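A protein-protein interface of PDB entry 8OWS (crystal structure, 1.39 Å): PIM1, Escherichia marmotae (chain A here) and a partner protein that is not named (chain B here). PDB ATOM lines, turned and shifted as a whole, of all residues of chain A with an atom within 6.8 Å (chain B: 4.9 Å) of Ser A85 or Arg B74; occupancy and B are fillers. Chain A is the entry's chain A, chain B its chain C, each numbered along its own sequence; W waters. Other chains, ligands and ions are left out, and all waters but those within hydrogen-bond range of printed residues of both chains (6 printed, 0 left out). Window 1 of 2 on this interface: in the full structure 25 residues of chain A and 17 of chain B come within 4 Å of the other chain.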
ATOM      1  N   ARG A  34      -9.732   2.361   2.108  1.00  0.00           N
ATOM      2  CA  ARG A  34     -10.495   2.634   3.321  1.00  0.00           C
ATOM      3  C   ARG A  34     -11.946   2.201   3.210  1.00  0.00           C
ATOM      4  O   ARG A  34     -12.574   1.897   4.236  1.00  0.00           O
ATOM      5  CB  ARG A  34     -10.446   4.116   3.661  1.00  0.00           C
ATOM      6  CG  ARG A  34      -9.071   4.583   4.153  1.00  0.00           C
ATOM      7  CD  ARG A  34      -9.051   6.042   4.525  1.00  0.00           C
ATOM      8  NE  ARG A  34      -9.966   6.347   5.636  1.00  0.00           N
ATOM      9  CZ  ARG A  34      -9.654   6.967   6.772  1.00  0.00           C
ATOM     10  NH1 ARG A  34      -8.410   7.362   7.040  1.00  0.00           N
ATOM     11  NH2 ARG A  34     -10.604   7.196   7.664  1.00  0.00           N
ATOM     12  N   ASP A  35     -12.491   2.151   1.992  1.00  0.00           N
ATOM     13  CA  ASP A  35     -13.870   1.714   1.813  1.00  0.00           C
ATOM     14  C   ASP A  35     -14.009   0.198   1.793  1.00  0.00           C
ATOM     15  O   ASP A  35     -15.141  -0.290   1.815  1.00  0.00           O
ATOM     16  CB  ASP A  35     -14.431   2.294   0.511  1.00  0.00           C
ATOM     17  CG  ASP A  35     -14.798   3.782   0.617  1.00  0.00           C
ATOM     18  OD1 ASP A  35     -14.756   4.363   1.724  1.00  0.00           O
ATOM     19  OD2 ASP A  35     -15.157   4.348  -0.434  1.00  0.00           O
ATOM     20  N   ASP A  40     -12.841  -0.512   6.732  1.00  0.00           N
ATOM     21  CA  ASP A  40     -14.139   0.094   7.042  1.00  0.00           C
ATOM     22  C   ASP A  40     -14.776  -0.547   8.272  1.00  0.00           C
ATOM     23  O   ASP A  40     -15.299   0.154   9.149  1.00  0.00           O
ATOM     24  CB  ASP A  40     -15.048  -0.023   5.820  1.00  0.00           C
ATOM     25  CG  ASP A  40     -16.337   0.745   5.969  1.00  0.00           C
ATOM     26  OD1 ASP A  40     -16.341   1.991   5.775  1.00  0.00           O
ATOM     27  OD2 ASP A  40     -17.385   0.140   6.295  1.00  0.00           O
ATOM     28  N   TRP A  43     -12.818   0.682  11.387  1.00  0.00           N
ATOM     29  CA  TRP A  43     -13.160   2.053  11.716  1.00  0.00           C
ATOM     30  C   TRP A  43     -14.530   2.116  12.378  1.00  0.00           C
ATOM     31  O   TRP A  43     -14.701   2.757  13.418  1.00  0.00           O
ATOM     32  CB  TRP A  43     -13.107   2.909  10.438  1.00  0.00           C
ATOM     33  CG  TRP A  43     -12.922   4.367  10.750  1.00  0.00           C
ATOM     34  CD1 TRP A  43     -11.751   5.077  10.674  1.00  0.00           C
ATOM     35  CD2 TRP A  43     -13.923   5.292  11.194  1.00  0.00           C
ATOM     36  NE1 TRP A  43     -11.963   6.385  11.060  1.00  0.00           N
ATOM     37  CE2 TRP A  43     -13.290   6.542  11.380  1.00  0.00           C
ATOM     38  CE3 TRP A  43     -15.288   5.192  11.449  1.00  0.00           C
ATOM     39  CZ2 TRP A  43     -13.963   7.655  11.826  1.00  0.00           C
ATOM     40  CZ3 TRP A  43     -15.966   6.330  11.874  1.00  0.00           C
ATOM     41  CH2 TRP A  43     -15.306   7.532  12.061  1.00  0.00           C
ATOM     42  N   MET A  44     -15.520   1.455  11.777  1.00  0.00           N
ATOM     43  CA  MET A  44     -16.861   1.483  12.350  1.00  0.00           C
ATOM     44  C   MET A  44     -16.919   0.818  13.717  1.00  0.00           C
ATOM     45  O   MET A  44     -17.670   1.276  14.578  1.00  0.00           O
ATOM     46  CB  MET A  44     -17.859   0.853  11.384  1.00  0.00           C
ATOM     47  CG  MET A  44     -18.169   1.719  10.151  1.00  0.00           C
ATOM     48  SD  MET A  44     -18.646   3.437  10.561  1.00  0.00           S
ATOM     49  CE  MET A  44     -20.046   3.152  11.629  1.00  0.00           C
ATOM     50  N   PHE A  71      -9.667  19.431   9.407  1.00  0.00           N
ATOM     51  CA  PHE A  71     -10.297  19.567   8.100  1.00  0.00           C
ATOM     52  C   PHE A  71      -9.618  20.660   7.284  1.00  0.00           C
ATOM     53  O   PHE A  71      -9.206  20.442   6.133  1.00  0.00           O
ATOM     54  CB  PHE A  71     -11.784  19.872   8.256  1.00  0.00           C
ATOM     55  CG  PHE A  71     -12.517  19.866   6.945  1.00  0.00           C
ATOM     56  CD1 PHE A  71     -13.201  18.733   6.520  1.00  0.00           C
ATOM     57  CD2 PHE A  71     -12.470  20.963   6.102  1.00  0.00           C
ATOM     58  CE1 PHE A  71     -13.817  18.702   5.276  1.00  0.00           C
ATOM     59  CE2 PHE A  71     -13.089  20.940   4.862  1.00  0.00           C
ATOM     60  CZ  PHE A  71     -13.781  19.807   4.459  1.00  0.00           C
ATOM     61  N   SER A  74      -5.725  20.356   6.438  1.00  0.00           N
ATOM     62  CA  SER A  74      -5.495  19.383   5.376  1.00  0.00           C
ATOM     63  C   SER A  74      -6.080  19.843   4.041  1.00  0.00           C
ATOM     64  O   SER A  74      -5.497  19.558   2.981  1.00  0.00           O
ATOM     65  CB  SER A  74      -6.040  18.020   5.790  1.00  0.00           C
ATOM     66  OG  SER A  74      -7.468  18.015   5.898  1.00  0.00           O
ATOM     67  N   ASN A  80      -9.081  18.561  -1.211  1.00  0.00           N
ATOM     68  CA  ASN A  80      -9.922  17.400  -1.458  1.00  0.00           C
ATOM     69  C   ASN A  80     -10.882  17.230  -0.290  1.00  0.00           C
ATOM     70  O   ASN A  80     -10.453  16.951   0.837  1.00  0.00           O
ATOM     71  CB  ASN A  80      -9.106  16.126  -1.674  1.00  0.00           C
ATOM     72  CG  ASN A  80      -9.969  14.973  -2.136  1.00  0.00           C
ATOM     73  OD1 ASN A  80     -10.780  14.453  -1.376  1.00  0.00           O
ATOM     74  ND2 ASN A  80      -9.818  14.576  -3.394  1.00  0.00           N
ATOM     75  N   ALA A  81     -12.181  17.388  -0.556  1.00  0.00           N
ATOM     76  CA  ALA A  81     -13.154  17.377   0.534  1.00  0.00           C
ATOM     77  C   ALA A  81     -13.260  16.017   1.213  1.00  0.00           C
ATOM     78  O   ALA A  81     -13.390  15.942   2.443  1.00  0.00           O
ATOM     79  CB  ALA A  81     -14.516  17.819  -0.002  1.00  0.00           C
ATOM     80  N   GLU A  82     -13.227  14.921   0.446  1.00  0.00           N
ATOM     81  CA  GLU A  82     -13.368  13.612   1.070  1.00  0.00           C
ATOM     82  C   GLU A  82     -12.172  13.302   1.962  1.00  0.00           C
ATOM     83  O   GLU A  82     -12.337  12.797   3.070  1.00  0.00           O
ATOM     84  CB  GLU A  82     -13.585  12.493   0.052  1.00  0.00           C
ATOM     85  CG  GLU A  82     -13.934  11.155   0.743  1.00  0.00           C
ATOM     86  CD  GLU A  82     -15.237  11.223   1.523  1.00  0.00           C
ATOM     87  OE1 GLU A  82     -16.130  12.026   1.164  1.00  0.00           O
ATOM     88  OE2 GLU A  82     -15.391  10.489   2.510  1.00  0.00           O
ATOM     89  N   ILE A  83     -10.954  13.589   1.492  1.00  0.00           N
ATOM     90  CA  ILE A  83      -9.785  13.399   2.336  1.00  0.00           C
ATOM     91  C   ILE A  83      -9.931  14.215   3.617  1.00  0.00           C
ATOM     92  O   ILE A  83      -9.757  13.707   4.730  1.00  0.00           O
ATOM     93  CB  ILE A  83      -8.498  13.756   1.568  1.00  0.00           C
ATOM     94  CG1 ILE A  83      -8.222  12.774   0.415  1.00  0.00           C
ATOM     95  CG2 ILE A  83      -7.320  13.784   2.548  1.00  0.00           C
ATOM     96  CD1 ILE A  83      -7.975  11.368   0.871  1.00  0.00           C
ATOM     97  N   SER A  84     -10.223  15.514   3.473  1.00  0.00           N
ATOM     98  CA  SER A  84     -10.318  16.371   4.656  1.00  0.00           C
ATOM     99  C   SER A  84     -11.423  15.902   5.599  1.00  0.00           C
ATOM    100  O   SER A  84     -11.260  15.937   6.828  1.00  0.00           O
ATOM    101  CB  SER A  84     -10.506  17.828   4.248  1.00  0.00           C
ATOM    102  OG  SER A  84      -9.291  18.312   3.657  1.00  0.00           O
ATOM    103  N   SER A  85     -12.544  15.428   5.035  1.00  0.00           N
ATOM    104  CA  SER A  85     -13.612  14.866   5.852  1.00  0.00           C
ATOM    105  C   SER A  85     -13.163  13.624   6.605  1.00  0.00           C
ATOM    106  O   SER A  85     -13.537  13.435   7.773  1.00  0.00           O
ATOM    107  CB  SER A  85     -14.810  14.510   4.980  1.00  0.00           C
ATOM    108  OG  SER A  85     -15.546  15.670   4.599  1.00  0.00           O
ATOM    109  N   ARG A  86     -12.406  12.740   5.951  1.00  0.00           N
ATOM    110  CA  ARG A  86     -11.972  11.518   6.625  1.00  0.00           C
ATOM    111  C   ARG A  86     -10.966  11.843   7.724  1.00  0.00           C
ATOM    112  O   ARG A  86     -10.980  11.225   8.788  1.00  0.00           O
ATOM    113  CB  ARG A  86     -11.395  10.530   5.607  1.00  0.00           C
ATOM    114  CG  ARG A  86     -12.420  10.156   4.542  1.00  0.00           C
ATOM    115  CD  ARG A  86     -12.784   8.706   4.566  1.00  0.00           C
ATOM    116  NE  ARG A  86     -13.752   8.472   3.499  1.00  0.00           N
ATOM    117  CZ  ARG A  86     -13.960   7.296   2.926  1.00  0.00           C
ATOM    118  NH1 ARG A  86     -13.328   6.206   3.352  1.00  0.00           N
ATOM    119  NH2 ARG A  86     -14.829   7.201   1.933  1.00  0.00           N
ATOM    120  N   ILE A  87     -10.108  12.841   7.493  1.00  0.00           N
ATOM    121  CA  ILE A  87      -9.145  13.255   8.506  1.00  0.00           C
ATOM    122  C   ILE A  87      -9.872  13.828   9.707  1.00  0.00           C
ATOM    123  O   ILE A  87      -9.552  13.497  10.849  1.00  0.00           O
ATOM    124  CB  ILE A  87      -8.146  14.256   7.895  1.00  0.00           C
ATOM    125  CG1 ILE A  87      -7.342  13.568   6.792  1.00  0.00           C
ATOM    126  CG2 ILE A  87      -7.239  14.843   8.972  1.00  0.00           C
ATOM    127  CD1 ILE A  87      -6.359  14.472   6.092  1.00  0.00           C
ATOM    128  N   SER A  88     -10.870  14.682   9.463  1.00  0.00           N
ATOM    129  CA  SER A  88     -11.698  15.217  10.546  1.00  0.00           C
ATOM    130  C   SER A  88     -12.346  14.101  11.364  1.00  0.00           C
ATOM    131  O   SER A  88     -12.261  14.084  12.600  1.00  0.00           O
ATOM    132  CB  SER A  88     -12.751  16.114   9.919  1.00  0.00           C
ATOM    133  OG  SER A  88     -13.608  16.651  10.903  1.00  0.00           O
ATOM    134  N   ASP A  89     -12.974  13.140  10.688  1.00  0.00           N
ATOM    135  CA  ASP A  89     -13.573  12.016  11.394  1.00  0.00           C
ATOM    136  C   ASP A  89     -12.520  11.225  12.171  1.00  0.00           C
ATOM    137  O   ASP A  89     -12.770  10.781  13.303  1.00  0.00           O
ATOM    138  CB  ASP A  89     -14.266  11.063  10.409  1.00  0.00           C
ATOM    139  CG  ASP A  89     -15.655  11.505   9.969  1.00  0.00           C
ATOM    140  OD1 ASP A  89     -16.073  12.668  10.119  1.00  0.00           O
ATOM    141  OD2 ASP A  89     -16.322  10.623   9.413  1.00  0.00           O
ATOM    142  N   ASP A  90     -11.348  10.990  11.554  1.00  0.00           N
ATOM    143  CA  ASP A  90     -10.285  10.276  12.261  1.00  0.00           C
ATOM    144  C   ASP A  90      -9.914  11.005  13.545  1.00  0.00           C
ATOM    145  O   ASP A  90      -9.776  10.399  14.617  1.00  0.00           O
ATOM    146  CB  ASP A  90      -9.042  10.149  11.367  1.00  0.00           C
ATOM    147  CG  ASP A  90      -9.174   9.097  10.267  1.00  0.00           C
ATOM    148  OD1 ASP A  90     -10.183   8.355  10.215  1.00  0.00           O
ATOM    149  OD2 ASP A  90      -8.243   9.033   9.425  1.00  0.00           O
ATOM    150  N   ALA B  28     -22.304  10.565  -1.349  1.00  0.00           N
ATOM    151  CA  ALA B  28     -20.911  10.197  -1.179  1.00  0.00           C
ATOM    152  C   ALA B  28     -20.633   8.813  -1.773  1.00  0.00           C
ATOM    153  O   ALA B  28     -21.497   7.943  -1.813  1.00  0.00           O
ATOM    154  CB  ALA B  28     -20.583  10.192   0.301  1.00  0.00           C
ATOM    155  N   ARG B  30     -18.819   6.256  -0.589  1.00  0.00           N
ATOM    156  CA  ARG B  30     -18.990   5.151   0.354  1.00  0.00           C
ATOM    157  C   ARG B  30     -20.455   4.861   0.603  1.00  0.00           C
ATOM    158  O   ARG B  30     -20.839   3.693   0.732  1.00  0.00           O
ATOM    159  CB  ARG B  30     -18.272   5.455   1.669  1.00  0.00           C
ATOM    160  CG  ARG B  30     -18.524   4.421   2.769  1.00  0.00           C
ATOM    161  CD  ARG B  30     -17.921   3.067   2.386  1.00  0.00           C
ATOM    162  NE  ARG B  30     -18.182   2.044   3.402  1.00  0.00           N
ATOM    163  CZ  ARG B  30     -19.304   1.324   3.458  1.00  0.00           C
ATOM    164  NH1 ARG B  30     -20.255   1.499   2.546  1.00  0.00           N
ATOM    165  NH2 ARG B  30     -19.472   0.426   4.427  1.00  0.00           N
ATOM    166  N   LYS B  31     -21.282   5.918   0.686  1.00  0.00           N
ATOM    167  CA  LYS B  31     -22.702   5.749   0.969  1.00  0.00           C
ATOM    168  C   LYS B  31     -23.467   5.205  -0.231  1.00  0.00           C
ATOM    169  O   LYS B  31     -24.573   4.666  -0.060  1.00  0.00           O
ATOM    170  CB  LYS B  31     -23.287   7.084   1.435  1.00  0.00           C
ATOM    171  CG  LYS B  31     -22.567   7.708   2.637  1.00  0.00           C
ATOM    172  CD  LYS B  31     -22.458   6.751   3.833  1.00  0.00           C
ATOM    173  CE  LYS B  31     -21.579   7.397   4.929  1.00  0.00           C
ATOM    174  NZ  LYS B  31     -21.520   6.559   6.169  1.00  0.00           N
ATOM    175  N   HIS B  64     -19.149  19.494   5.187  1.00  0.00           N
ATOM    176  CA  HIS B  64     -18.715  18.336   5.961  1.00  0.00           C
ATOM    177  C   HIS B  64     -19.477  18.237   7.268  1.00  0.00           C
ATOM    178  O   HIS B  64     -19.961  17.159   7.649  1.00  0.00           O
ATOM    179  CB  HIS B  64     -17.209  18.427   6.273  1.00  0.00           C
ATOM    180  CG  HIS B  64     -16.789  17.531   7.404  1.00  0.00           C
ATOM    181  ND1 HIS B  64     -16.655  16.168   7.266  1.00  0.00           N
ATOM    182  CD2 HIS B  64     -16.550  17.796   8.712  1.00  0.00           C
ATOM    183  CE1 HIS B  64     -16.340  15.634   8.433  1.00  0.00           C
ATOM    184  NE2 HIS B  64     -16.269  16.596   9.327  1.00  0.00           N
ATOM    185  N   GLU B  67     -23.150  17.282   6.888  1.00  0.00           N
ATOM    186  CA  GLU B  67     -23.274  15.868   6.546  1.00  0.00           C
ATOM    187  C   GLU B  67     -22.907  14.979   7.731  1.00  0.00           C
ATOM    188  O   GLU B  67     -23.543  13.932   7.948  1.00  0.00           O
ATOM    189  CB  GLU B  67     -22.410  15.560   5.323  1.00  0.00           C
ATOM    190  CG  GLU B  67     -22.881  16.240   4.062  1.00  0.00           C
ATOM    191  CD  GLU B  67     -22.064  15.868   2.829  1.00  0.00           C
ATOM    192  OE1 GLU B  67     -21.463  14.778   2.811  1.00  0.00           O
ATOM    193  OE2 GLU B  67     -22.017  16.655   1.868  1.00  0.00           O
ATOM    194  N   GLY B  72     -23.806  11.064   9.079  1.00  0.00           N
ATOM    195  CA  GLY B  72     -22.940  10.411  10.026  1.00  0.00           C
ATOM    196  C   GLY B  72     -21.502  10.384   9.561  1.00  0.00           C
ATOM    197  O   GLY B  72     -21.046  11.249   8.807  1.00  0.00           O
ATOM    198  N   PRO B  73     -20.757   9.390  10.027  1.00  0.00           N
ATOM    199  CA  PRO B  73     -19.351   9.286   9.625  1.00  0.00           C
ATOM    200  C   PRO B  73     -19.207   9.048   8.130  1.00  0.00           C
ATOM    201  O   PRO B  73     -20.113   8.552   7.462  1.00  0.00           O
ATOM    202  CB  PRO B  73     -18.840   8.081  10.432  1.00  0.00           C
ATOM    203  CG  PRO B  73     -20.022   7.300  10.737  1.00  0.00           C
ATOM    204  CD  PRO B  73     -21.177   8.263  10.883  1.00  0.00           C
ATOM    205  N   ARG B  74     -18.033   9.400   7.585  1.00  0.00           N
ATOM    206  CA  ARG B  74     -17.758   9.110   6.186  1.00  0.00           C
ATOM    207  C   ARG B  74     -17.669   7.605   5.931  1.00  0.00           C
ATOM    208  O   ARG B  74     -18.050   7.141   4.851  1.00  0.00           O
ATOM    209  CB  ARG B  74     -16.396   9.731   5.793  1.00  0.00           C
ATOM    210  CG  ARG B  74     -16.260  11.231   6.096  1.00  0.00           C
ATOM    211  CD  ARG B  74     -17.415  12.131   5.538  1.00  0.00           C
ATOM    212  NE  ARG B  74     -17.501  12.095   4.091  1.00  0.00           N
ATOM    213  CZ  ARG B  74     -18.403  12.808   3.413  1.00  0.00           C
ATOM    214  NH1 ARG B  74     -19.236  13.595   4.086  1.00  0.00           N
ATOM    215  NH2 ARG B  74     -18.463  12.709   2.091  1.00  0.00           N
ATOM    216  N   GLN B  75     -17.158   6.841   6.903  1.00  0.00           N
ATOM    217  CA  GLN B  75     -17.065   5.398   6.769  1.00  0.00           C
ATOM    218  C   GLN B  75     -18.429   4.776   7.060  1.00  0.00           C
ATOM    219  O   GLN B  75     -19.356   5.421   7.573  1.00  0.00           O
ATOM    220  CB  GLN B  75     -16.017   4.827   7.748  1.00  0.00           C
ATOM    221  CG  GLN B  75     -14.593   5.439   7.608  1.00  0.00           C
ATOM    222  CD  GLN B  75     -13.766   4.919   6.432  1.00  0.00           C
ATOM    223  OE1 GLN B  75     -12.763   5.544   6.091  1.00  0.00           O
ATOM    224  NE2 GLN B  75     -14.106   3.758   5.871  1.00  0.00           N
ATOM    225  N   GLY B  76     -18.553   3.501   6.714  1.00  0.00           N
ATOM    226  CA  GLY B  76     -19.746   2.754   7.039  1.00  0.00           C
ATOM    227  C   GLY B  76     -20.882   2.955   6.041  1.00  0.00           C
ATOM    228  O   GLY B  76     -20.955   3.927   5.298  1.00  0.00           O
HETATM  229  O   HOH W   1     -15.544   8.075   9.032  1.00  0.00           O
HETATM  230  O   HOH W   2     -18.520  12.802   8.599  1.00  0.00           O
HETATM  231  O   HOH W   3     -18.401   8.966   2.820  1.00  0.00           O
HETATM  232  O   HOH W   4     -16.525  14.552   0.391  1.00  0.00           O
HETATM  233  O   HOH W   5     -18.202  12.989  -0.984  1.00  0.00           O
HETATM  234  O   HOH W   6     -17.083   8.440   0.371  1.00  0.00           O
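The backbone carbonyl oxygen of Arg A34 lies within hydrogen-bond range of the side-chain amide nitrogen of Gln B75 (2.9 Å). The guanidinium group (NH2) of Arg B30 lies within salt-bridge range of the side-chain carboxylate (OD2) of Asp A40 (2.8 Å). OD1 of Asp A40 is in hydrogen-bond range of NE2 of Gln B75, 2.9 Å away. The side-chain carboxylate (OD1) of Asp A40 sits at hydrogen-bond distance from the backbone NH (N) of Gly B76, 2.8 Å away. The side-chain carboxylate (OE1) of Glu A82 lies within salt-bridge range of the guanidinium group (NH2) of Arg B74 (2.6 Å). A ring nitrogen (ND1) of His B64 sits at hydrogen-bond distance from the side-chain hydroxyl (OG) of Ser A85, at 2.9 Å. NH1 of Arg A86 sits at hydrogen-bond distance from OE1 of Gln B75. The side-chain hydroxyl (OG) of Ser A88 lies within hydrogen-bond range of a ring nitrogen (NE2) of His B64 (3.1 Å). The backbone NH (N) of Arg B74 is in hydrogen-bond range of the side-chain carboxylate (OD2) of Asp A89 (2.8 Å). The side-chain sulfur (SD) of Met A44 lies close to the backbone carbonyl oxygen (O) of Gln B75 (3.7 Å).
The side-chain carboxylate of Asp A35 lies within salt-bridge range of the guanidinium group of Arg A86 (2.8 Å). OG of Ser A84 lies within hydrogen-bond range of O of Phe A71, 3.3 Å away. The backbone NH of Glu A82 lies within hydrogen-bond range of the side-chain amide oxygen of Asn A80. The guanidinium group (NE) of Arg A86 lies within salt-bridge range of the side-chain carboxylate (OE2) of Glu A82. The side-chain amino group (NZ) of Lys B31 sits at hydrogen-bond distance from the backbone carbonyl oxygen (O) of Pro B73 (2.8 Å). The side-chain amino group (NZ) of Lys B31 is in hydrogen-bond range of the backbone carbonyl oxygen (O) of Gln B75 (2.8 Å).
Asp A35 touches Arg B30 (OD1 to CD, 3.5 Å). Trp A43 touches Pro B73 (CZ3 to CB, 3.7 Å). CD2 of Trp A43 touches CG of Gln B75 (3.7 Å). Met A44 touches Gly B76 (CG to CA, 3.6 Å). His B64 touches Phe A71 (CB to CE1, 3.5 Å). Arg B74 touches Ser A85 (CD to CB, 3.6 Å). Arg A86 touches Arg B30. Arg A86 touches Arg B74 (NE to CB, 3.7 Å). Asp A89 touches His B64. Asp A89 touches Pro B73 (OD2 to CA, 3.3 Å).
Of the printed residues of chain B, Glu A82 touches Arg B74. Ser A84 touches none of the printed residues of chain B. Ser A85 touches two residues of chain B. Of the printed residues of chain B, Ser A88 touches His B64. Arg B74 touches four residues of chain A. The nearest printed residue of chain B that does not touch Ser A85 is Glu B67 (6.2 Å). The nearest printed residue of chain A that does not touch Arg B30 is Arg A34 (5.7 Å).
Of the 10 printed residues of chain B, 6 touch a printed residue of chain A. Printed residues of chain B that touch a printed residue of chain A: Arg B30, His B64, Pro B73, Arg B74, Gln B75 and Gly B76. Hydrophobic or aromatic side chains of chain B that line the printed part of chain A: His B64 and Pro B73. Along chain B the printed residues that touch a printed residue of chain A span positions 30 to 76. Along chain A the printed residues that touch a printed residue of chain B span positions 34 to 89. Among the printed residues, Asp or Glu carboxylates within 4 Å of a Lys or Arg side-chain nitrogen of the other chain: Asp A40 with Arg B30 (2.8 Å) and Glu A82 with Arg B74 (2.6 Å).
Water W4 lies within hydrogen-bond range of the side-chain carboxylate (OE1) of Glu A82 (2.7 Å) and the guanidinium group (NH2) of Arg B74 (3.2 Å). Water W1 lies within hydrogen-bond range of the side-chain carboxylate (OD2) of Asp A89, the backbone NH (N) of Gln B75 and the backbone NH (N) of Arg B74. Water W3 lies within hydrogen-bond range of O of Arg B74 (2.8 Å) and OE2 of Glu A82 (3.4 Å). Water W2 bridges the side-chain carboxylate of Asp A89 and the backbone carbonyl oxygen of Gly B72. Water W6 lies within hydrogen-bond range of N of Arg B30 (3.0 Å), NH2 of Arg A86 (3.0 Å) and OE2 of Glu A82 (3.4 Å). Water W5 lies within hydrogen-bond range of NH2 of Arg B74 (3.1 Å) and OE1 of Glu A82 (3.1 Å).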
